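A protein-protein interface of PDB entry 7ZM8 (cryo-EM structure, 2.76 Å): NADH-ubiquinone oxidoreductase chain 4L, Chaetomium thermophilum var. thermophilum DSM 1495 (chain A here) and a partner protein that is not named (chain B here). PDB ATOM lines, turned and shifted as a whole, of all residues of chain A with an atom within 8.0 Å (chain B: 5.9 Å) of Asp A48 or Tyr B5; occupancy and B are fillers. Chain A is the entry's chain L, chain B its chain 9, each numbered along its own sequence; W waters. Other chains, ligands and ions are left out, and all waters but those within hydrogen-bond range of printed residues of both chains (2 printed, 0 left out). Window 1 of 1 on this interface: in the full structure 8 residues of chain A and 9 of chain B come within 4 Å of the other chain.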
ATOM      1  N   LEU A  42      30.048  24.386 -37.746  1.00  0.00           N
ATOM      2  CA  LEU A  42      31.058  23.820 -36.811  1.00  0.00           C
ATOM      3  C   LEU A  42      31.099  24.696 -35.565  1.00  0.00           C
ATOM      4  O   LEU A  42      31.255  24.142 -34.482  1.00  0.00           O
ATOM      5  CB  LEU A  42      32.434  23.757 -37.480  1.00  0.00           C
ATOM      6  CG  LEU A  42      32.604  22.772 -38.629  1.00  0.00           C
ATOM      7  CD1 LEU A  42      34.077  22.525 -38.895  1.00  0.00           C
ATOM      8  CD2 LEU A  42      31.902  21.472 -38.321  1.00  0.00           C
ATOM      9  N   SER A  43      30.944  26.006 -35.722  1.00  0.00           N
ATOM     10  CA  SER A  43      30.853  26.858 -34.548  1.00  0.00           C
ATOM     11  C   SER A  43      29.546  26.664 -33.803  1.00  0.00           C
ATOM     12  O   SER A  43      29.454  27.027 -32.628  1.00  0.00           O
ATOM     13  CB  SER A  43      31.011  28.321 -34.956  1.00  0.00           C
ATOM     14  OG  SER A  43      32.186  28.504 -35.725  1.00  0.00           O
ATOM     15  N   SER A  44      28.511  26.193 -34.470  1.00  0.00           N
ATOM     16  CA  SER A  44      27.193  25.930 -33.836  1.00  0.00           C
ATOM     17  C   SER A  44      27.301  24.727 -32.901  1.00  0.00           C
ATOM     18  O   SER A  44      26.827  24.834 -31.772  1.00  0.00           O
ATOM     19  CB  SER A  44      26.152  25.768 -34.881  1.00  0.00           C
ATOM     20  OG  SER A  44      26.085  26.939 -35.670  1.00  0.00           O
ATOM     21  N   LEU A  45      27.913  23.637 -33.361  1.00  0.00           N
ATOM     22  CA  LEU A  45      28.168  22.450 -32.508  1.00  0.00           C
ATOM     23  C   LEU A  45      29.058  22.847 -31.320  1.00  0.00           C
ATOM     24  O   LEU A  45      28.894  22.247 -30.253  1.00  0.00           O
ATOM     25  CB  LEU A  45      28.824  21.384 -33.391  1.00  0.00           C
ATOM     26  CG  LEU A  45      28.960  19.987 -32.797  1.00  0.00           C
ATOM     27  CD1 LEU A  45      27.596  19.340 -32.640  1.00  0.00           C
ATOM     28  CD2 LEU A  45      29.849  19.132 -33.682  1.00  0.00           C
ATOM     29  N   ASN A  46      29.929  23.839 -31.474  1.00  0.00           N
ATOM     30  CA  ASN A  46      30.874  24.195 -30.383  1.00  0.00           C
ATOM     31  C   ASN A  46      30.180  25.045 -29.328  1.00  0.00           C
ATOM     32  O   ASN A  46      30.677  25.044 -28.206  1.00  0.00           O
ATOM     33  CB  ASN A  46      32.090  24.964 -30.905  1.00  0.00           C
ATOM     34  CG  ASN A  46      33.004  24.130 -31.772  1.00  0.00           C
ATOM     35  OD1 ASN A  46      32.928  22.905 -31.772  1.00  0.00           O
ATOM     36  ND2 ASN A  46      33.873  24.789 -32.517  1.00  0.00           N
ATOM     37  N   MET A  47      29.025  25.640 -29.636  1.00  0.00           N
ATOM     38  CA  MET A  47      28.315  26.542 -28.692  1.00  0.00           C
ATOM     39  C   MET A  47      26.945  25.988 -28.316  1.00  0.00           C
ATOM     40  O   MET A  47      26.221  26.713 -27.627  1.00  0.00           O
ATOM     41  CB  MET A  47      28.153  27.926 -29.322  1.00  0.00           C
ATOM     42  CG  MET A  47      29.459  28.579 -29.730  1.00  0.00           C
ATOM     43  SD  MET A  47      29.252  30.250 -30.414  1.00  0.00           S
ATOM     44  CE  MET A  47      27.965  29.977 -31.627  1.00  0.00           C
ATOM     45  N   ASP A  48      26.617  24.759 -28.709  1.00  0.00           N
ATOM     46  CA  ASP A  48      25.307  24.107 -28.420  1.00  0.00           C
ATOM     47  C   ASP A  48      24.150  24.986 -28.878  1.00  0.00           C
ATOM     48  O   ASP A  48      23.213  25.165 -28.101  1.00  0.00           O
ATOM     49  CB  ASP A  48      25.149  23.706 -26.955  1.00  0.00           C
ATOM     50  CG  ASP A  48      24.030  22.709 -26.712  1.00  0.00           C
ATOM     51  OD1 ASP A  48      24.055  21.639 -27.348  1.00  0.00           O
ATOM     52  OD2 ASP A  48      23.133  23.017 -25.897  1.00  0.00           O
ATOM     53  N   ASP A  49      24.220  25.512 -30.091  1.00  0.00           N
ATOM     54  CA  ASP A  49      23.183  26.465 -30.555  1.00  0.00           C
ATOM     55  C   ASP A  49      22.522  25.913 -31.815  1.00  0.00           C
ATOM     56  O   ASP A  49      23.215  25.730 -32.816  1.00  0.00           O
ATOM     57  CB  ASP A  49      23.784  27.856 -30.746  1.00  0.00           C
ATOM     58  CG  ASP A  49      22.815  28.983 -30.439  1.00  0.00           C
ATOM     59  OD1 ASP A  49      21.671  28.676 -30.055  1.00  0.00           O
ATOM     60  OD2 ASP A  49      23.214  30.157 -30.587  1.00  0.00           O
ATOM     61  N   ILE A  50      21.223  25.666 -31.757  1.00  0.00           N
ATOM     62  CA  ILE A  50      20.502  25.168 -32.923  1.00  0.00           C
ATOM     63  C   ILE A  50      20.201  26.266 -33.927  1.00  0.00           C
ATOM     64  O   ILE A  50      19.787  25.966 -35.051  1.00  0.00           O
ATOM     65  CB  ILE A  50      19.199  24.471 -32.482  1.00  0.00           C
ATOM     66  CG1 ILE A  50      18.757  23.432 -33.518  1.00  0.00           C
ATOM     67  CG2 ILE A  50      18.100  25.486 -32.252  1.00  0.00           C
ATOM     68  CD1 ILE A  50      19.604  22.186 -33.550  1.00  0.00           C
ATOM     69  N   ILE A  51      20.408  27.532 -33.560  1.00  0.00           N
ATOM     70  CA  ILE A  51      20.081  28.626 -34.466  1.00  0.00           C
ATOM     71  C   ILE A  51      21.117  28.729 -35.574  1.00  0.00           C
ATOM     72  O   ILE A  51      20.833  29.240 -36.663  1.00  0.00           O
ATOM     73  CB  ILE A  51      19.949  29.946 -33.687  1.00  0.00           C
ATOM     74  CG1 ILE A  51      19.176  30.974 -34.505  1.00  0.00           C
ATOM     75  CG2 ILE A  51      21.312  30.498 -33.337  1.00  0.00           C
ATOM     76  CD1 ILE A  51      18.748  32.164 -33.715  1.00  0.00           C
ATOM     77  N   GLY A  52      22.336  28.253 -35.314  1.00  0.00           N
ATOM     78  CA  GLY A  52      23.325  28.176 -36.372  1.00  0.00           C
ATOM     79  C   GLY A  52      22.944  27.174 -37.442  1.00  0.00           C
ATOM     80  O   GLY A  52      23.198  27.388 -38.626  1.00  0.00           O
ATOM     81  N   GLN A  53      22.338  26.062 -37.034  1.00  0.00           N
ATOM     82  CA  GLN A  53      21.861  25.079 -37.996  1.00  0.00           C
ATOM     83  C   GLN A  53      20.739  25.648 -38.846  1.00  0.00           C
ATOM     84  O   GLN A  53      20.596  25.290 -40.018  1.00  0.00           O
ATOM     85  CB  GLN A  53      21.392  23.829 -37.263  1.00  0.00           C
ATOM     86  CG  GLN A  53      22.454  23.173 -36.434  1.00  0.00           C
ATOM     87  CD  GLN A  53      22.283  21.682 -36.367  1.00  0.00           C
ATOM     88  OE1 GLN A  53      21.677  21.081 -37.244  1.00  0.00           O
ATOM     89  NE2 GLN A  53      22.809  21.074 -35.318  1.00  0.00           N
ATOM     90  N   SER B   3      20.885  32.229 -28.142  1.00  0.00           N
ATOM     91  CA  SER B   3      19.515  32.140 -28.708  1.00  0.00           C
ATOM     92  C   SER B   3      18.625  31.547 -27.627  1.00  0.00           C
ATOM     93  O   SER B   3      17.488  32.008 -27.476  1.00  0.00           O
ATOM     94  CB  SER B   3      19.455  31.325 -29.951  1.00  0.00           C
ATOM     95  OG  SER B   3      19.439  29.941 -29.661  1.00  0.00           O
ATOM     96  N   GLY B   4      19.169  30.617 -26.864  1.00  0.00           N
ATOM     97  CA  GLY B   4      18.398  29.948 -25.840  1.00  0.00           C
ATOM     98  C   GLY B   4      17.840  28.608 -26.250  1.00  0.00           C
ATOM     99  O   GLY B   4      17.123  27.991 -25.459  1.00  0.00           O
ATOM    100  N   TYR B   5      18.126  28.144 -27.459  1.00  0.00           N
ATOM    101  CA  TYR B   5      17.678  26.847 -27.940  1.00  0.00           C
ATOM    102  C   TYR B   5      18.900  26.034 -28.333  1.00  0.00           C
ATOM    103  O   TYR B   5      19.743  26.505 -29.101  1.00  0.00           O
ATOM    104  CB  TYR B   5      16.703  27.012 -29.112  1.00  0.00           C
ATOM    105  CG  TYR B   5      15.590  27.972 -28.782  1.00  0.00           C
ATOM    106  CD1 TYR B   5      15.729  29.329 -29.016  1.00  0.00           C
ATOM    107  CD2 TYR B   5      14.417  27.529 -28.188  1.00  0.00           C
ATOM    108  CE1 TYR B   5      14.735  30.210 -28.688  1.00  0.00           C
ATOM    109  CE2 TYR B   5      13.407  28.407 -27.865  1.00  0.00           C
ATOM    110  CZ  TYR B   5      13.575  29.749 -28.113  1.00  0.00           C
ATOM    111  OH  TYR B   5      12.582  30.640 -27.789  1.00  0.00           O
ATOM    112  N   GLY B   6      19.020  24.837 -27.772  1.00  0.00           N
ATOM    113  CA  GLY B   6      20.175  23.971 -28.038  1.00  0.00           C
ATOM    114  C   GLY B   6      19.871  22.843 -28.988  1.00  0.00           C
ATOM    115  O   GLY B   6      18.733  22.750 -29.448  1.00  0.00           O
ATOM    116  N   LEU B   7      20.858  21.996 -29.240  1.00  0.00           N
ATOM    117  CA  LEU B   7      20.731  20.900 -30.226  1.00  0.00           C
ATOM    118  C   LEU B   7      19.770  19.787 -29.801  1.00  0.00           C
ATOM    119  O   LEU B   7      19.231  19.141 -30.704  1.00  0.00           O
ATOM    120  CB  LEU B   7      22.142  20.377 -30.506  1.00  0.00           C
ATOM    121  CG  LEU B   7      23.218  21.439 -30.725  1.00  0.00           C
ATOM    122  CD1 LEU B   7      24.586  20.795 -30.855  1.00  0.00           C
ATOM    123  CD2 LEU B   7      22.917  22.271 -31.954  1.00  0.00           C
ATOM    124  N   ASN B   8      19.533  19.580 -28.505  1.00  0.00           N
ATOM    125  CA  ASN B   8      18.765  18.404 -28.015  1.00  0.00           C
ATOM    126  C   ASN B   8      17.326  18.713 -27.618  1.00  0.00           C
ATOM    127  O   ASN B   8      16.732  17.891 -26.910  1.00  0.00           O
ATOM    128  CB  ASN B   8      19.429  17.808 -26.778  1.00  0.00           C
ATOM    129  CG  ASN B   8      19.303  18.711 -25.569  1.00  0.00           C
ATOM    130  OD1 ASN B   8      19.691  19.877 -25.613  1.00  0.00           O
ATOM    131  ND2 ASN B   8      18.742  18.186 -24.495  1.00  0.00           N
ATOM    132  N   GLY B  10      16.750  21.851 -26.383  1.00  0.00           N
ATOM    133  CA  GLY B  10      16.926  23.118 -25.656  1.00  0.00           C
ATOM    134  C   GLY B  10      17.223  22.957 -24.199  1.00  0.00           C
ATOM    135  O   GLY B  10      16.987  21.824 -23.763  1.00  0.00           O
ATOM    136  N   PRO B  11      17.629  24.008 -23.414  1.00  0.00           N
ATOM    137  CA  PRO B  11      18.168  25.276 -23.917  1.00  0.00           C
ATOM    138  C   PRO B  11      19.645  25.204 -24.280  1.00  0.00           C
ATOM    139  O   PRO B  11      20.230  24.128 -24.199  1.00  0.00           O
ATOM    140  CB  PRO B  11      17.956  26.232 -22.741  1.00  0.00           C
ATOM    141  CG  PRO B  11      17.043  25.508 -21.801  1.00  0.00           C
ATOM    142  CD  PRO B  11      17.378  24.081 -21.970  1.00  0.00           C
ATOM    143  N   SER B  12      20.207  26.374 -24.628  1.00  0.00           N
ATOM    144  CA  SER B  12      21.635  26.466 -25.037  1.00  0.00           C
ATOM    145  C   SER B  12      22.556  26.619 -23.825  1.00  0.00           C
ATOM    146  O   SER B  12      22.163  27.294 -22.893  1.00  0.00           O
ATOM    147  CB  SER B  12      21.859  27.505 -26.108  1.00  0.00           C
ATOM    148  OG  SER B  12      21.303  28.755 -25.766  1.00  0.00           O
ATOM    149  N   ARG B  13      23.765  26.062 -23.873  1.00  0.00           N
ATOM    150  CA  ARG B  13      24.679  26.030 -22.693  1.00  0.00           C
ATOM    151  C   ARG B  13      25.097  27.411 -22.200  1.00  0.00           C
ATOM    152  O   ARG B  13      25.260  27.555 -20.989  1.00  0.00           O
ATOM    153  CB  ARG B  13      25.901  25.142 -22.951  1.00  0.00           C
ATOM    154  CG  ARG B  13      26.678  25.458 -24.215  1.00  0.00           C
ATOM    155  CD  ARG B  13      27.897  24.565 -24.279  1.00  0.00           C
ATOM    156  NE  ARG B  13      28.807  25.097 -25.272  1.00  0.00           N
ATOM    157  CZ  ARG B  13      29.760  25.967 -24.994  1.00  0.00           C
ATOM    158  NH1 ARG B  13      30.541  26.424 -25.955  1.00  0.00           N
ATOM    159  NH2 ARG B  13      29.927  26.375 -23.752  1.00  0.00           N
ATOM    160  N   PHE B  15      23.461  30.275 -22.694  1.00  0.00           N
ATOM    161  CA  PHE B  15      22.307  31.192 -22.514  1.00  0.00           C
ATOM    162  C   PHE B  15      22.250  31.769 -21.090  1.00  0.00           C
ATOM    163  O   PHE B  15      21.929  32.953 -20.977  1.00  0.00           O
ATOM    164  CB  PHE B  15      21.017  30.539 -23.004  1.00  0.00           C
ATOM    165  CG  PHE B  15      19.809  31.436 -23.016  1.00  0.00           C
ATOM    166  CD1 PHE B  15      19.734  32.505 -23.891  1.00  0.00           C
ATOM    167  CD2 PHE B  15      18.742  31.200 -22.168  1.00  0.00           C
ATOM    168  CE1 PHE B  15      18.616  33.320 -23.916  1.00  0.00           C
ATOM    169  CE2 PHE B  15      17.626  32.018 -22.194  1.00  0.00           C
ATOM    170  CZ  PHE B  15      17.564  33.071 -23.073  1.00  0.00           C
HETATM  171  O   HOH W   1      29.519  22.643 -26.979  1.00  0.00           O
HETATM  172  O   HOH W   2      22.335  19.682 -27.071  1.00  0.00           O
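Water W2 lies within hydrogen-bond range of the side-chain carboxylate (OD1) of Asp A48 (2.6 Å), the side-chain amide oxygen (OD1) of Asn B8 (3.0 Å) and the backbone NH (N) of Leu B7 (3.5 Å). Water W1 lies within hydrogen-bond range of the backbone carbonyl oxygen of Asn A46 (2.9 Å), the guanidinium group of Arg B13 (3.1 Å) and the backbone carbonyl oxygen of Leu A45 (3.4 Å).
Of the 12 printed residues of chain A, 8 touch a printed residue of chain B. Printed residues of chain B that touch a printed residue of chain A: Ser B3, Tyr B5, Gly B6, Leu B7, Pro B11, Ser B12 and Arg B13. Among the printed residues, no Asp or Glu carboxylate lies within 4 Å of a Lys or Arg side-chain nitrogen of the other chain.
Of chain B, only Tyr B5, Gly B6, Leu B7, Pro B11, Ser B12 and Arg B13 come within 4 Å of Asp A48. Tyr B5 touches just these residues of chain A: Asp A48, Asp A49 and Ile A50. No residue of chain A comes within 4 Å of Gly B4. Gly B6 touches just these residues of chain A: Asp A48 and Ile A50. Printed residues of chain A within 4 Å of Ser B12: Asp A48. Printed residues of chain A within 4 Å of Arg B13: Asn A46, Met A47 and Asp A48. Of the printed residues of chain A, Ser B3 touches Asp A49 (2.6 Å) and Ile A51 (3.9 Å). Printed residues of chain B within 4 Å of Met A47: Arg B13.
The side-chain amide nitrogen of Asn A46 lies close to the backbone carbonyl oxygen of Leu A42 (3.3 Å). The backbone NH (N) of Asp A49 is in hydrogen-bond range of the backbone carbonyl oxygen (O) of Ser A44 (3.2 Å). OG of Ser B3 sits at hydrogen-bond distance from N of Tyr B5 (3.1 Å). The backbone NH (N) of Gly B4 is in hydrogen-bond range of the side-chain hydroxyl (OG) of Ser B12, 3.0 Å away.
Among the printed residues, merely in contact across the chains: Leu A45 with Leu B7, Met A47 with Arg B13, Asp A48 with Tyr B5, Asp A48 with Gly B6, Asp A48 with Leu B7, Asp A48 with Pro B11, Asp A48 with Ser B12, Asp A48 with Arg B13, Asp A49 with Leu B7, Ile A50 with Gly B6, Ile A50 with Leu B7, Ile A51 with Ser B3 and Gln A53 with Leu B7.
O of Asn A46 is in hydrogen-bond range of NH1 of Arg B13, at 2.6 Å. The side-chain carboxylate of Asp A49 is in hydrogen-bond range of the side-chain hydroxyl of Ser B3 (2.6 Å). The backbone NH of Ile A50 sits at hydrogen-bond distance from the backbone carbonyl oxygen of Tyr B5, at 3.2 Å. The backbone carbonyl oxygen of Tyr B5 sits close to the side-chain carboxylate of Asp A49 (3.1 Å).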
